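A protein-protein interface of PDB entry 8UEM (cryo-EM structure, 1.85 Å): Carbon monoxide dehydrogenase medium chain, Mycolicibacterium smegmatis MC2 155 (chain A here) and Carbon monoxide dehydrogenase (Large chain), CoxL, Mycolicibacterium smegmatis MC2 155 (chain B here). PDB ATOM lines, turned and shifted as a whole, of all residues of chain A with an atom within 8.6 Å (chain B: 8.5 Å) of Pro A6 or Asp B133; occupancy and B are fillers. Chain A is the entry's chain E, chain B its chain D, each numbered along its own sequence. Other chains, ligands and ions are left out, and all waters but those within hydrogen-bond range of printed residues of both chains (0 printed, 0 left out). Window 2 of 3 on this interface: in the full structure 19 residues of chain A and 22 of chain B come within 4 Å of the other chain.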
ATOM      1  N   GLN A   2      29.138  10.206   0.464  1.00  0.00           N
ATOM      2  CA  GLN A   2      28.569   8.936   0.041  1.00  0.00           C
ATOM      3  C   GLN A   2      27.282   8.684   0.809  1.00  0.00           C
ATOM      4  O   GLN A   2      27.241   8.833   2.031  1.00  0.00           O
ATOM      5  CB  GLN A   2      29.559   7.802   0.274  1.00  0.00           C
ATOM      6  CG  GLN A   2      30.756   7.827  -0.647  1.00  0.00           C
ATOM      7  CD  GLN A   2      31.767   6.761  -0.303  1.00  0.00           C
ATOM      8  OE1 GLN A   2      31.540   5.578  -0.538  1.00  0.00           O
ATOM      9  NE2 GLN A   2      32.887   7.173   0.269  1.00  0.00           N
ATOM     10  N   VAL A   3      26.232   8.305   0.093  1.00  0.00           N
ATOM     11  CA  VAL A   3      24.911   8.164   0.700  1.00  0.00           C
ATOM     12  C   VAL A   3      24.375   6.774   0.389  1.00  0.00           C
ATOM     13  O   VAL A   3      24.786   6.130  -0.588  1.00  0.00           O
ATOM     14  CB  VAL A   3      23.937   9.258   0.209  1.00  0.00           C
ATOM     15  CG1 VAL A   3      24.320  10.608   0.794  1.00  0.00           C
ATOM     16  CG2 VAL A   3      23.913   9.299  -1.305  1.00  0.00           C
ATOM     17  N   PRO A   4      23.462   6.280   1.212  1.00  0.00           N
ATOM     18  CA  PRO A   4      22.938   4.927   1.010  1.00  0.00           C
ATOM     19  C   PRO A   4      22.091   4.828  -0.249  1.00  0.00           C
ATOM     20  O   PRO A   4      21.529   5.807  -0.740  1.00  0.00           O
ATOM     21  CB  PRO A   4      22.090   4.681   2.262  1.00  0.00           C
ATOM     22  CG  PRO A   4      22.467   5.763   3.230  1.00  0.00           C
ATOM     23  CD  PRO A   4      22.900   6.923   2.408  1.00  0.00           C
ATOM     24  N   GLY A   5      22.004   3.610  -0.768  1.00  0.00           N
ATOM     25  CA  GLY A   5      21.030   3.302  -1.783  1.00  0.00           C
ATOM     26  C   GLY A   5      19.640   3.303  -1.183  1.00  0.00           C
ATOM     27  O   GLY A   5      19.473   3.310   0.040  1.00  0.00           O
ATOM     28  N   PRO A   6      18.612   3.307  -2.026  1.00  0.00           N
ATOM     29  CA  PRO A   6      17.243   3.311  -1.502  1.00  0.00           C
ATOM     30  C   PRO A   6      16.968   2.076  -0.658  1.00  0.00           C
ATOM     31  O   PRO A   6      17.486   0.990  -0.915  1.00  0.00           O
ATOM     32  CB  PRO A   6      16.376   3.330  -2.764  1.00  0.00           C
ATOM     33  CG  PRO A   6      17.268   3.847  -3.833  1.00  0.00           C
ATOM     34  CD  PRO A   6      18.641   3.371  -3.495  1.00  0.00           C
ATOM     35  N   PHE A   7      16.126   2.252   0.355  1.00  0.00           N
ATOM     36  CA  PHE A   7      15.683   1.122   1.207  1.00  0.00           C
ATOM     37  C   PHE A   7      14.356   1.552   1.825  1.00  0.00           C
ATOM     38  O   PHE A   7      13.995   2.720   1.725  1.00  0.00           O
ATOM     39  CB  PHE A   7      16.724   0.740   2.268  1.00  0.00           C
ATOM     40  CG  PHE A   7      17.054   1.807   3.279  1.00  0.00           C
ATOM     41  CD1 PHE A   7      16.311   1.944   4.438  1.00  0.00           C
ATOM     42  CD2 PHE A   7      18.118   2.666   3.073  1.00  0.00           C
ATOM     43  CE1 PHE A   7      16.614   2.927   5.363  1.00  0.00           C
ATOM     44  CE2 PHE A   7      18.428   3.639   4.007  1.00  0.00           C
ATOM     45  CZ  PHE A   7      17.675   3.770   5.146  1.00  0.00           C
ATOM     46  N   GLU A   8      13.701   0.641   2.519  1.00  0.00           N
ATOM     47  CA  GLU A   8      12.416   0.970   3.161  1.00  0.00           C
ATOM     48  C   GLU A   8      12.691   1.031   4.652  1.00  0.00           C
ATOM     49  O   GLU A   8      13.618   0.381   5.127  1.00  0.00           O
ATOM     50  CB  GLU A   8      11.289   0.015   2.742  1.00  0.00           C
ATOM     51  CG  GLU A   8      10.904   0.175   1.286  1.00  0.00           C
ATOM     52  CD  GLU A   8      10.315   1.538   0.971  1.00  0.00           C
ATOM     53  OE1 GLU A   8      10.953   2.298   0.224  1.00  0.00           O
ATOM     54  OE2 GLU A   8       9.215   1.831   1.477  1.00  0.00           O
ATOM     55  N   TYR A   9      11.965   1.880   5.334  1.00  0.00           N
ATOM     56  CA  TYR A   9      12.245   2.070   6.763  1.00  0.00           C
ATOM     57  C   TYR A   9      11.048   1.634   7.593  1.00  0.00           C
ATOM     58  O   TYR A   9       9.931   1.984   7.247  1.00  0.00           O
ATOM     59  CB  TYR A   9      12.569   3.537   7.027  1.00  0.00           C
ATOM     60  CG  TYR A   9      12.751   3.933   8.465  1.00  0.00           C
ATOM     61  CD1 TYR A   9      13.996   3.876   9.063  1.00  0.00           C
ATOM     62  CD2 TYR A   9      11.689   4.411   9.211  1.00  0.00           C
ATOM     63  CE1 TYR A   9      14.179   4.266  10.375  1.00  0.00           C
ATOM     64  CE2 TYR A   9      11.851   4.798  10.525  1.00  0.00           C
ATOM     65  CZ  TYR A   9      13.100   4.729  11.104  1.00  0.00           C
ATOM     66  OH  TYR A   9      13.253   5.119  12.393  1.00  0.00           O
ATOM     67  N   MET A  42      26.155   1.169   4.474  1.00  0.00           N
ATOM     68  CA  MET A  42      25.188   1.493   3.430  1.00  0.00           C
ATOM     69  C   MET A  42      25.581   2.763   2.690  1.00  0.00           C
ATOM     70  O   MET A  42      25.408   2.854   1.472  1.00  0.00           O
ATOM     71  CB  MET A  42      23.783   1.621   4.019  1.00  0.00           C
ATOM     72  CG  MET A  42      23.427   0.541   5.018  1.00  0.00           C
ATOM     73  SD  MET A  42      21.823   0.782   5.798  1.00  0.00           S
ATOM     74  CE  MET A  42      20.886   1.542   4.479  1.00  0.00           C
ATOM     75  N   LYS A  43      26.119   3.748   3.405  1.00  0.00           N
ATOM     76  CA  LYS A  43      26.607   4.950   2.743  1.00  0.00           C
ATOM     77  C   LYS A  43      27.695   4.600   1.742  1.00  0.00           C
ATOM     78  O   LYS A  43      27.758   5.179   0.654  1.00  0.00           O
ATOM     79  CB  LYS A  43      27.123   5.954   3.774  1.00  0.00           C
ATOM     80  CG  LYS A  43      26.038   6.688   4.545  1.00  0.00           C
ATOM     81  CD  LYS A  43      26.534   7.174   5.902  1.00  0.00           C
ATOM     82  CE  LYS A  43      27.395   8.420   5.761  1.00  0.00           C
ATOM     83  NZ  LYS A  43      27.847   8.950   7.072  1.00  0.00           N
ATOM     84  N   ARG A  45      27.725   1.749   0.408  1.00  0.00           N
ATOM     85  CA  ARG A  45      27.058   0.789  -0.455  1.00  0.00           C
ATOM     86  C   ARG A  45      27.687  -0.590  -0.347  1.00  0.00           C
ATOM     87  O   ARG A  45      27.543  -1.420  -1.248  1.00  0.00           O
ATOM     88  CB  ARG A  45      27.048   1.281  -1.904  1.00  0.00           C
ATOM     89  CG  ARG A  45      25.851   2.164  -2.222  1.00  0.00           C
ATOM     90  CD  ARG A  45      26.219   3.328  -3.112  1.00  0.00           C
ATOM     91  NE  ARG A  45      25.321   4.458  -2.915  1.00  0.00           N
ATOM     92  CZ  ARG A  45      24.104   4.549  -3.429  1.00  0.00           C
ATOM     93  NH1 ARG A  45      23.603   3.590  -4.190  1.00  0.00           N
ATOM     94  NH2 ARG A  45      23.371   5.628  -3.176  1.00  0.00           N
ATOM     95  N   ALA A  47      26.755  -2.404   2.365  1.00  0.00           N
ATOM     96  CA  ALA A  47      25.524  -3.021   2.833  1.00  0.00           C
ATOM     97  C   ALA A  47      24.356  -2.364   2.117  1.00  0.00           C
ATOM     98  O   ALA A  47      24.284  -1.134   2.039  1.00  0.00           O
ATOM     99  CB  ALA A  47      25.374  -2.874   4.347  1.00  0.00           C
ATOM    100  N   ASN A  48      23.462  -3.179   1.574  1.00  0.00           N
ATOM    101  CA  ASN A  48      22.293  -2.686   0.845  1.00  0.00           C
ATOM    102  C   ASN A  48      21.047  -3.430   1.302  1.00  0.00           C
ATOM    103  O   ASN A  48      20.408  -4.143   0.525  1.00  0.00           O
ATOM    104  CB  ASN A  48      22.507  -2.823  -0.660  1.00  0.00           C
ATOM    105  CG  ASN A  48      23.818  -2.212  -1.114  1.00  0.00           C
ATOM    106  OD1 ASN A  48      23.863  -1.061  -1.541  1.00  0.00           O
ATOM    107  ND2 ASN A  48      24.898  -2.975  -1.004  1.00  0.00           N
ATOM    108  N   PRO A  49      20.675  -3.290   2.570  1.00  0.00           N
ATOM    109  CA  PRO A  49      19.423  -3.892   3.033  1.00  0.00           C
ATOM    110  C   PRO A  49      18.234  -3.298   2.294  1.00  0.00           C
ATOM    111  O   PRO A  49      18.196  -2.103   2.005  1.00  0.00           O
ATOM    112  CB  PRO A  49      19.393  -3.539   4.524  1.00  0.00           C
ATOM    113  CG  PRO A  49      20.262  -2.324   4.637  1.00  0.00           C
ATOM    114  CD  PRO A  49      21.339  -2.504   3.625  1.00  0.00           C
ATOM    115  N   GLU A  50      17.258  -4.148   1.978  1.00  0.00           N
ATOM    116  CA  GLU A  50      16.007  -3.625   1.438  1.00  0.00           C
ATOM    117  C   GLU A  50      15.209  -2.895   2.507  1.00  0.00           C
ATOM    118  O   GLU A  50      14.531  -1.909   2.208  1.00  0.00           O
ATOM    119  CB  GLU A  50      15.174  -4.748   0.825  1.00  0.00           C
ATOM    120  CG  GLU A  50      15.967  -5.687  -0.063  1.00  0.00           C
ATOM    121  CD  GLU A  50      16.528  -4.998  -1.287  1.00  0.00           C
ATOM    122  OE1 GLU A  50      17.300  -4.032  -1.126  1.00  0.00           O
ATOM    123  OE2 GLU A  50      16.204  -5.426  -2.418  1.00  0.00           O
ATOM    124  N   TYR A  51      15.380  -3.338   3.731  1.00  0.00           N
ATOM    125  CA  TYR A  51      14.567  -2.755   4.816  1.00  0.00           C
ATOM    126  C   TYR A  51      15.419  -2.552   6.058  1.00  0.00           C
ATOM    127  O   TYR A  51      16.284  -3.358   6.301  1.00  0.00           O
ATOM    128  CB  TYR A  51      13.425  -3.692   5.222  1.00  0.00           C
ATOM    129  CG  TYR A  51      12.617  -4.297   4.106  1.00  0.00           C
ATOM    130  CD1 TYR A  51      11.533  -3.626   3.566  1.00  0.00           C
ATOM    131  CD2 TYR A  51      12.926  -5.546   3.595  1.00  0.00           C
ATOM    132  CE1 TYR A  51      10.786  -4.173   2.539  1.00  0.00           C
ATOM    133  CE2 TYR A  51      12.189  -6.110   2.567  1.00  0.00           C
ATOM    134  CZ  TYR A  51      11.115  -5.419   2.039  1.00  0.00           C
ATOM    135  OH  TYR A  51      10.378  -5.962   1.026  1.00  0.00           O
ATOM    136  N   LEU A  52      15.192  -1.446   6.749  1.00  0.00           N
ATOM    137  CA  LEU A  52      15.813  -1.250   8.067  1.00  0.00           C
ATOM    138  C   LEU A  52      14.708  -1.258   9.099  1.00  0.00           C
ATOM    139  O   LEU A  52      13.767  -0.493   8.979  1.00  0.00           O
ATOM    140  CB  LEU A  52      16.583   0.068   8.205  1.00  0.00           C
ATOM    141  CG  LEU A  52      17.918   0.141   7.477  1.00  0.00           C
ATOM    142  CD1 LEU A  52      18.665   1.397   7.892  1.00  0.00           C
ATOM    143  CD2 LEU A  52      18.744  -1.095   7.775  1.00  0.00           C
ATOM    144  N   ALA B  55      27.450  13.960  -9.537  1.00  0.00           N
ATOM    145  CA  ALA B  55      28.272  12.952  -8.892  1.00  0.00           C
ATOM    146  C   ALA B  55      29.207  12.373  -9.937  1.00  0.00           C
ATOM    147  O   ALA B  55      28.814  12.178 -11.082  1.00  0.00           O
ATOM    148  CB  ALA B  55      27.420  11.847  -8.258  1.00  0.00           C
ATOM    149  N   ALA B  73      21.920   2.723 -18.583  1.00  0.00           N
ATOM    150  CA  ALA B  73      21.123   2.512 -17.378  1.00  0.00           C
ATOM    151  C   ALA B  73      21.101   3.760 -16.505  1.00  0.00           C
ATOM    152  O   ALA B  73      20.047   4.144 -15.989  1.00  0.00           O
ATOM    153  CB  ALA B  73      21.654   1.311 -16.598  1.00  0.00           C
ATOM    154  N   ALA B  74      22.252   4.412 -16.332  1.00  0.00           N
ATOM    155  CA  ALA B  74      22.280   5.649 -15.559  1.00  0.00           C
ATOM    156  C   ALA B  74      21.437   6.727 -16.227  1.00  0.00           C
ATOM    157  O   ALA B  74      20.721   7.471 -15.552  1.00  0.00           O
ATOM    158  CB  ALA B  74      23.721   6.124 -15.370  1.00  0.00           C
ATOM    159  N   HIS B  77      17.756   6.401 -15.563  1.00  0.00           N
ATOM    160  CA  HIS B  77      17.286   6.733 -14.229  1.00  0.00           C
ATOM    161  C   HIS B  77      16.327   7.916 -14.314  1.00  0.00           C
ATOM    162  O   HIS B  77      16.679   8.951 -14.895  1.00  0.00           O
ATOM    163  CB  HIS B  77      18.473   7.066 -13.329  1.00  0.00           C
ATOM    164  CG  HIS B  77      18.148   7.087 -11.870  1.00  0.00           C
ATOM    165  ND1 HIS B  77      17.364   8.063 -11.298  1.00  0.00           N
ATOM    166  CD2 HIS B  77      18.526   6.268 -10.861  1.00  0.00           C
ATOM    167  CE1 HIS B  77      17.264   7.840 -10.000  1.00  0.00           C
ATOM    168  NE2 HIS B  77      17.957   6.754  -9.710  1.00  0.00           N
ATOM    169  N   LYS B  79      15.503  10.211 -12.394  1.00  0.00           N
ATOM    170  CA  LYS B  79      15.967  11.435 -11.757  1.00  0.00           C
ATOM    171  C   LYS B  79      17.282  11.940 -12.331  1.00  0.00           C
ATOM    172  O   LYS B  79      17.762  12.994 -11.908  1.00  0.00           O
ATOM    173  CB  LYS B  79      16.106  11.209 -10.250  1.00  0.00           C
ATOM    174  CG  LYS B  79      14.880  11.638  -9.474  1.00  0.00           C
ATOM    175  CD  LYS B  79      15.172  11.773  -7.992  1.00  0.00           C
ATOM    176  CE  LYS B  79      13.924  11.507  -7.175  1.00  0.00           C
ATOM    177  NZ  LYS B  79      13.233  12.772  -6.806  1.00  0.00           N
ATOM    178  N   VAL B  80      17.866  11.229 -13.286  1.00  0.00           N
ATOM    179  CA  VAL B  80      19.161  11.591 -13.845  1.00  0.00           C
ATOM    180  C   VAL B  80      18.930  12.469 -15.063  1.00  0.00           C
ATOM    181  O   VAL B  80      18.221  12.080 -15.994  1.00  0.00           O
ATOM    182  CB  VAL B  80      19.981  10.345 -14.205  1.00  0.00           C
ATOM    183  CG1 VAL B  80      21.132  10.706 -15.130  1.00  0.00           C
ATOM    184  CG2 VAL B  80      20.497   9.681 -12.945  1.00  0.00           C
ATOM    185  N   VAL B 123      27.381  12.107 -13.506  1.00  0.00           N
ATOM    186  CA  VAL B 123      25.937  12.089 -13.657  1.00  0.00           C
ATOM    187  C   VAL B 123      25.386  13.334 -12.990  1.00  0.00           C
ATOM    188  O   VAL B 123      25.704  13.617 -11.831  1.00  0.00           O
ATOM    189  CB  VAL B 123      25.318  10.824 -13.038  1.00  0.00           C
ATOM    190  CG1 VAL B 123      23.808  10.934 -13.028  1.00  0.00           C
ATOM    191  CG2 VAL B 123      25.775   9.594 -13.792  1.00  0.00           C
ATOM    192  N   ALA B 125      21.906  14.731 -11.721  1.00  0.00           N
ATOM    193  CA  ALA B 125      20.636  14.173 -11.302  1.00  0.00           C
ATOM    194  C   ALA B 125      19.901  15.205 -10.463  1.00  0.00           C
ATOM    195  O   ALA B 125      20.452  16.239 -10.084  1.00  0.00           O
ATOM    196  CB  ALA B 125      20.838  12.872 -10.520  1.00  0.00           C
ATOM    197  N   ASP B 127      18.885  15.161  -7.368  1.00  0.00           N
ATOM    198  CA  ASP B 127      19.422  15.354  -6.030  1.00  0.00           C
ATOM    199  C   ASP B 127      20.683  14.517  -5.872  1.00  0.00           C
ATOM    200  O   ASP B 127      20.977  13.642  -6.686  1.00  0.00           O
ATOM    201  CB  ASP B 127      18.388  14.997  -4.961  1.00  0.00           C
ATOM    202  CG  ASP B 127      18.267  13.508  -4.755  1.00  0.00           C
ATOM    203  OD1 ASP B 127      17.704  12.841  -5.641  1.00  0.00           O
ATOM    204  OD2 ASP B 127      18.738  13.002  -3.717  1.00  0.00           O
ATOM    205  N   ARG B 128      21.434  14.800  -4.807  1.00  0.00           N
ATOM    206  CA  ARG B 128      22.703  14.106  -4.605  1.00  0.00           C
ATOM    207  C   ARG B 128      22.498  12.603  -4.494  1.00  0.00           C
ATOM    208  O   ARG B 128      23.243  11.818  -5.094  1.00  0.00           O
ATOM    209  CB  ARG B 128      23.408  14.637  -3.358  1.00  0.00           C
ATOM    210  CG  ARG B 128      22.471  15.123  -2.279  1.00  0.00           C
ATOM    211  CD  ARG B 128      23.225  15.505  -1.011  1.00  0.00           C
ATOM    212  NE  ARG B 128      24.513  16.120  -1.297  1.00  0.00           N
ATOM    213  CZ  ARG B 128      24.751  17.423  -1.255  1.00  0.00           C
ATOM    214  NH1 ARG B 128      23.802  18.291  -0.947  1.00  0.00           N
ATOM    215  NH2 ARG B 128      25.971  17.869  -1.530  1.00  0.00           N
ATOM    216  N   TYR B 129      21.480  12.183  -3.741  1.00  0.00           N
ATOM    217  CA  TYR B 129      21.262  10.757  -3.525  1.00  0.00           C
ATOM    218  C   TYR B 129      21.017  10.038  -4.843  1.00  0.00           C
ATOM    219  O   TYR B 129      21.630   9.001  -5.127  1.00  0.00           O
ATOM    220  CB  TYR B 129      20.091  10.543  -2.564  1.00  0.00           C
ATOM    221  CG  TYR B 129      20.408  10.846  -1.116  1.00  0.00           C
ATOM    222  CD1 TYR B 129      20.618  12.145  -0.679  1.00  0.00           C
ATOM    223  CD2 TYR B 129      20.494   9.823  -0.184  1.00  0.00           C
ATOM    224  CE1 TYR B 129      20.911  12.412   0.641  1.00  0.00           C
ATOM    225  CE2 TYR B 129      20.781  10.082   1.135  1.00  0.00           C
ATOM    226  CZ  TYR B 129      20.990  11.376   1.544  1.00  0.00           C
ATOM    227  OH  TYR B 129      21.279  11.632   2.857  1.00  0.00           O
ATOM    228  N   SER B 130      20.120  10.582  -5.663  1.00  0.00           N
ATOM    229  CA  SER B 130      19.847   9.972  -6.955  1.00  0.00           C
ATOM    230  C   SER B 130      21.090   9.980  -7.832  1.00  0.00           C
ATOM    231  O   SER B 130      21.329   9.034  -8.585  1.00  0.00           O
ATOM    232  CB  SER B 130      18.681  10.690  -7.634  1.00  0.00           C
ATOM    233  OG  SER B 130      19.132  11.706  -8.501  1.00  0.00           O
ATOM    234  N   ALA B 131      21.902  11.035  -7.739  1.00  0.00           N
ATOM    235  CA  ALA B 131      23.122  11.096  -8.538  1.00  0.00           C
ATOM    236  C   ALA B 131      24.057   9.941  -8.198  1.00  0.00           C
ATOM    237  O   ALA B 131      24.594   9.272  -9.092  1.00  0.00           O
ATOM    238  CB  ALA B 131      23.820  12.440  -8.324  1.00  0.00           C
ATOM    239  N   ARG B 132      24.256   9.689  -6.904  1.00  0.00           N
ATOM    240  CA  ARG B 132      25.094   8.564  -6.488  1.00  0.00           C
ATOM    241  C   ARG B 132      24.503   7.226  -6.930  1.00  0.00           C
ATOM    242  O   ARG B 132      25.227   6.347  -7.429  1.00  0.00           O
ATOM    243  CB  ARG B 132      25.280   8.590  -4.974  1.00  0.00           C
ATOM    244  CG  ARG B 132      25.795   9.911  -4.429  1.00  0.00           C
ATOM    245  CD  ARG B 132      27.172   9.753  -3.820  1.00  0.00           C
ATOM    246  NE  ARG B 132      28.010  10.934  -3.978  1.00  0.00           N
ATOM    247  CZ  ARG B 132      29.295  10.900  -4.301  1.00  0.00           C
ATOM    248  NH1 ARG B 132      29.911   9.760  -4.561  1.00  0.00           N
ATOM    249  NH2 ARG B 132      29.981  12.038  -4.357  1.00  0.00           N
ATOM    250  N   ASP B 133      23.191   7.048  -6.756  1.00  0.00           N
ATOM    251  CA  ASP B 133      22.548   5.841  -7.272  1.00  0.00           C
ATOM    252  C   ASP B 133      22.884   5.644  -8.745  1.00  0.00           C
ATOM    253  O   ASP B 133      23.289   4.556  -9.180  1.00  0.00           O
ATOM    254  CB  ASP B 133      21.031   5.930  -7.102  1.00  0.00           C
ATOM    255  CG  ASP B 133      20.612   6.225  -5.688  1.00  0.00           C
ATOM    256  OD1 ASP B 133      21.434   6.080  -4.764  1.00  0.00           O
ATOM    257  OD2 ASP B 133      19.446   6.617  -5.496  1.00  0.00           O
ATOM    258  N   ALA B 134      22.731   6.709  -9.526  1.00  0.00           N
ATOM    259  CA  ALA B 134      22.967   6.611 -10.956  1.00  0.00           C
ATOM    260  C   ALA B 134      24.397   6.194 -11.237  1.00  0.00           C
ATOM    261  O   ALA B 134      24.648   5.357 -12.111  1.00  0.00           O
ATOM    262  CB  ALA B 134      22.656   7.942 -11.629  1.00  0.00           C
ATOM    263  N   LEU B 135      25.351   6.776 -10.511  1.00  0.00           N
ATOM    264  CA  LEU B 135      26.737   6.348 -10.649  1.00  0.00           C
ATOM    265  C   LEU B 135      26.829   4.842 -10.512  1.00  0.00           C
ATOM    266  O   LEU B 135      27.478   4.165 -11.317  1.00  0.00           O
ATOM    267  CB  LEU B 135      27.613   7.021  -9.596  1.00  0.00           C
ATOM    268  CG  LEU B 135      27.954   8.496  -9.765  1.00  0.00           C
ATOM    269  CD1 LEU B 135      29.103   8.824  -8.836  1.00  0.00           C
ATOM    270  CD2 LEU B 135      28.305   8.831 -11.199  1.00  0.00           C
ATOM    271  N   GLU B 136      26.159   4.299  -9.496  1.00  0.00           N
ATOM    272  CA  GLU B 136      26.096   2.848  -9.379  1.00  0.00           C
ATOM    273  C   GLU B 136      25.583   2.222 -10.667  1.00  0.00           C
ATOM    274  O   GLU B 136      26.040   1.146 -11.066  1.00  0.00           O
ATOM    275  CB  GLU B 136      25.204   2.446  -8.207  1.00  0.00           C
ATOM    276  CG  GLU B 136      25.719   2.872  -6.854  1.00  0.00           C
ATOM    277  CD  GLU B 136      27.191   2.582  -6.655  1.00  0.00           C
ATOM    278  OE1 GLU B 136      27.657   1.507  -7.083  1.00  0.00           O
ATOM    279  OE2 GLU B 136      27.880   3.431  -6.055  1.00  0.00           O
ATOM    280  N   LEU B 137      24.652   2.891 -11.346  1.00  0.00           N
ATOM    281  CA  LEU B 137      24.090   2.320 -12.569  1.00  0.00           C
ATOM    282  C   LEU B 137      25.068   2.291 -13.743  1.00  0.00           C
ATOM    283  O   LEU B 137      24.829   1.558 -14.705  1.00  0.00           O
ATOM    284  CB  LEU B 137      22.837   3.085 -12.980  1.00  0.00           C
ATOM    285  CG  LEU B 137      21.655   2.899 -12.033  1.00  0.00           C
ATOM    286  CD1 LEU B 137      20.453   3.685 -12.519  1.00  0.00           C
ATOM    287  CD2 LEU B 137      21.332   1.427 -11.923  1.00  0.00           C
ATOM    288  N   ILE B 138      26.140   3.067 -13.711  1.00  0.00           N
ATOM    289  CA  ILE B 138      27.029   3.150 -14.866  1.00  0.00           C
ATOM    290  C   ILE B 138      27.931   1.927 -14.919  1.00  0.00           C
ATOM    291  O   ILE B 138      28.477   1.488 -13.901  1.00  0.00           O
ATOM    292  CB  ILE B 138      27.856   4.444 -14.832  1.00  0.00           C
ATOM    293  CG1 ILE B 138      26.948   5.654 -15.034  1.00  0.00           C
ATOM    294  CG2 ILE B 138      28.943   4.392 -15.898  1.00  0.00           C
ATOM    295  CD1 ILE B 138      27.634   6.977 -14.799  1.00  0.00           C
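The side-chain carboxylate (OD1) of Asp B133 lies within salt-bridge range of the guanidinium group (NH2) of Arg A45 (2.5 Å).
The side-chain carboxylate of Asp B127 lies within hydrogen-bond range of the backbone NH of Tyr B129.
The backbone carbonyl oxygen (O) of Val A3 lies within hydrogen-bond range of the guanidinium group (NE) of Arg A45, 2.9 Å away.
The backbone carbonyl oxygen (O) of Pro A4 is in hydrogen-bond range of the guanidinium group (NH2) of Arg A45 (3.1 Å).
The side-chain amide nitrogen (ND2) of Asn A48 sits at hydrogen-bond distance from the backbone carbonyl oxygen (O) of Arg A45 (3.1 Å).
CE2 of Tyr B129 touches CB of Val A3, 3.4 Å away.
CG2 of Val A3 touches CG of Arg B132, at 3.7 Å.
Asp B133 touches Pro A6.
Arg B132 touches Arg A45.
OE2 of Glu B136 touches CD of Arg A45, 3.4 Å away.
Of chain B, only Asp B133 (3.9 Å) comes within 4 Å of Pro A6.
No residue of chain B comes within 4 Å of Gly A5.
No residue of chain A comes within 4 Å of Ala B134.
Of the printed residues of chain B, Val A3 touches Tyr B129 and Arg B132.
Of the printed residues of chain A, Glu B136 touches Arg A45 (3.4 Å).
Printed residues of chain A within 4 Å of Arg B132: Val A3 and Arg A45.
Printed residues of chain A within 4 Å of Tyr B129: Val A3 (3.4 Å).
Asp B127 touches none of the printed residues of chain A.
Ser B130 touches none of the printed residues of chain A.
The nearest printed residue of chain B that does not touch Pro A6 is Tyr B129 (6.6 Å).
The nearest residue of chain A that does not touch Asp B133 is Pro A4 (4.03 Å).
The nearest printed residue of chain A that does not touch Tyr B129 is Pro A4 (4.01 Å).
Hydrophobic or aromatic side chains of chain B within 4 Å of the printed part of chain A: Tyr B129.
Among the printed residues, 6 pairs touch across the chains.
Among the printed residues, Asp or Glu carboxylates within 4 Å of a Lys or Arg side-chain nitrogen of the other chain: Arg A45 with Asp B133.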
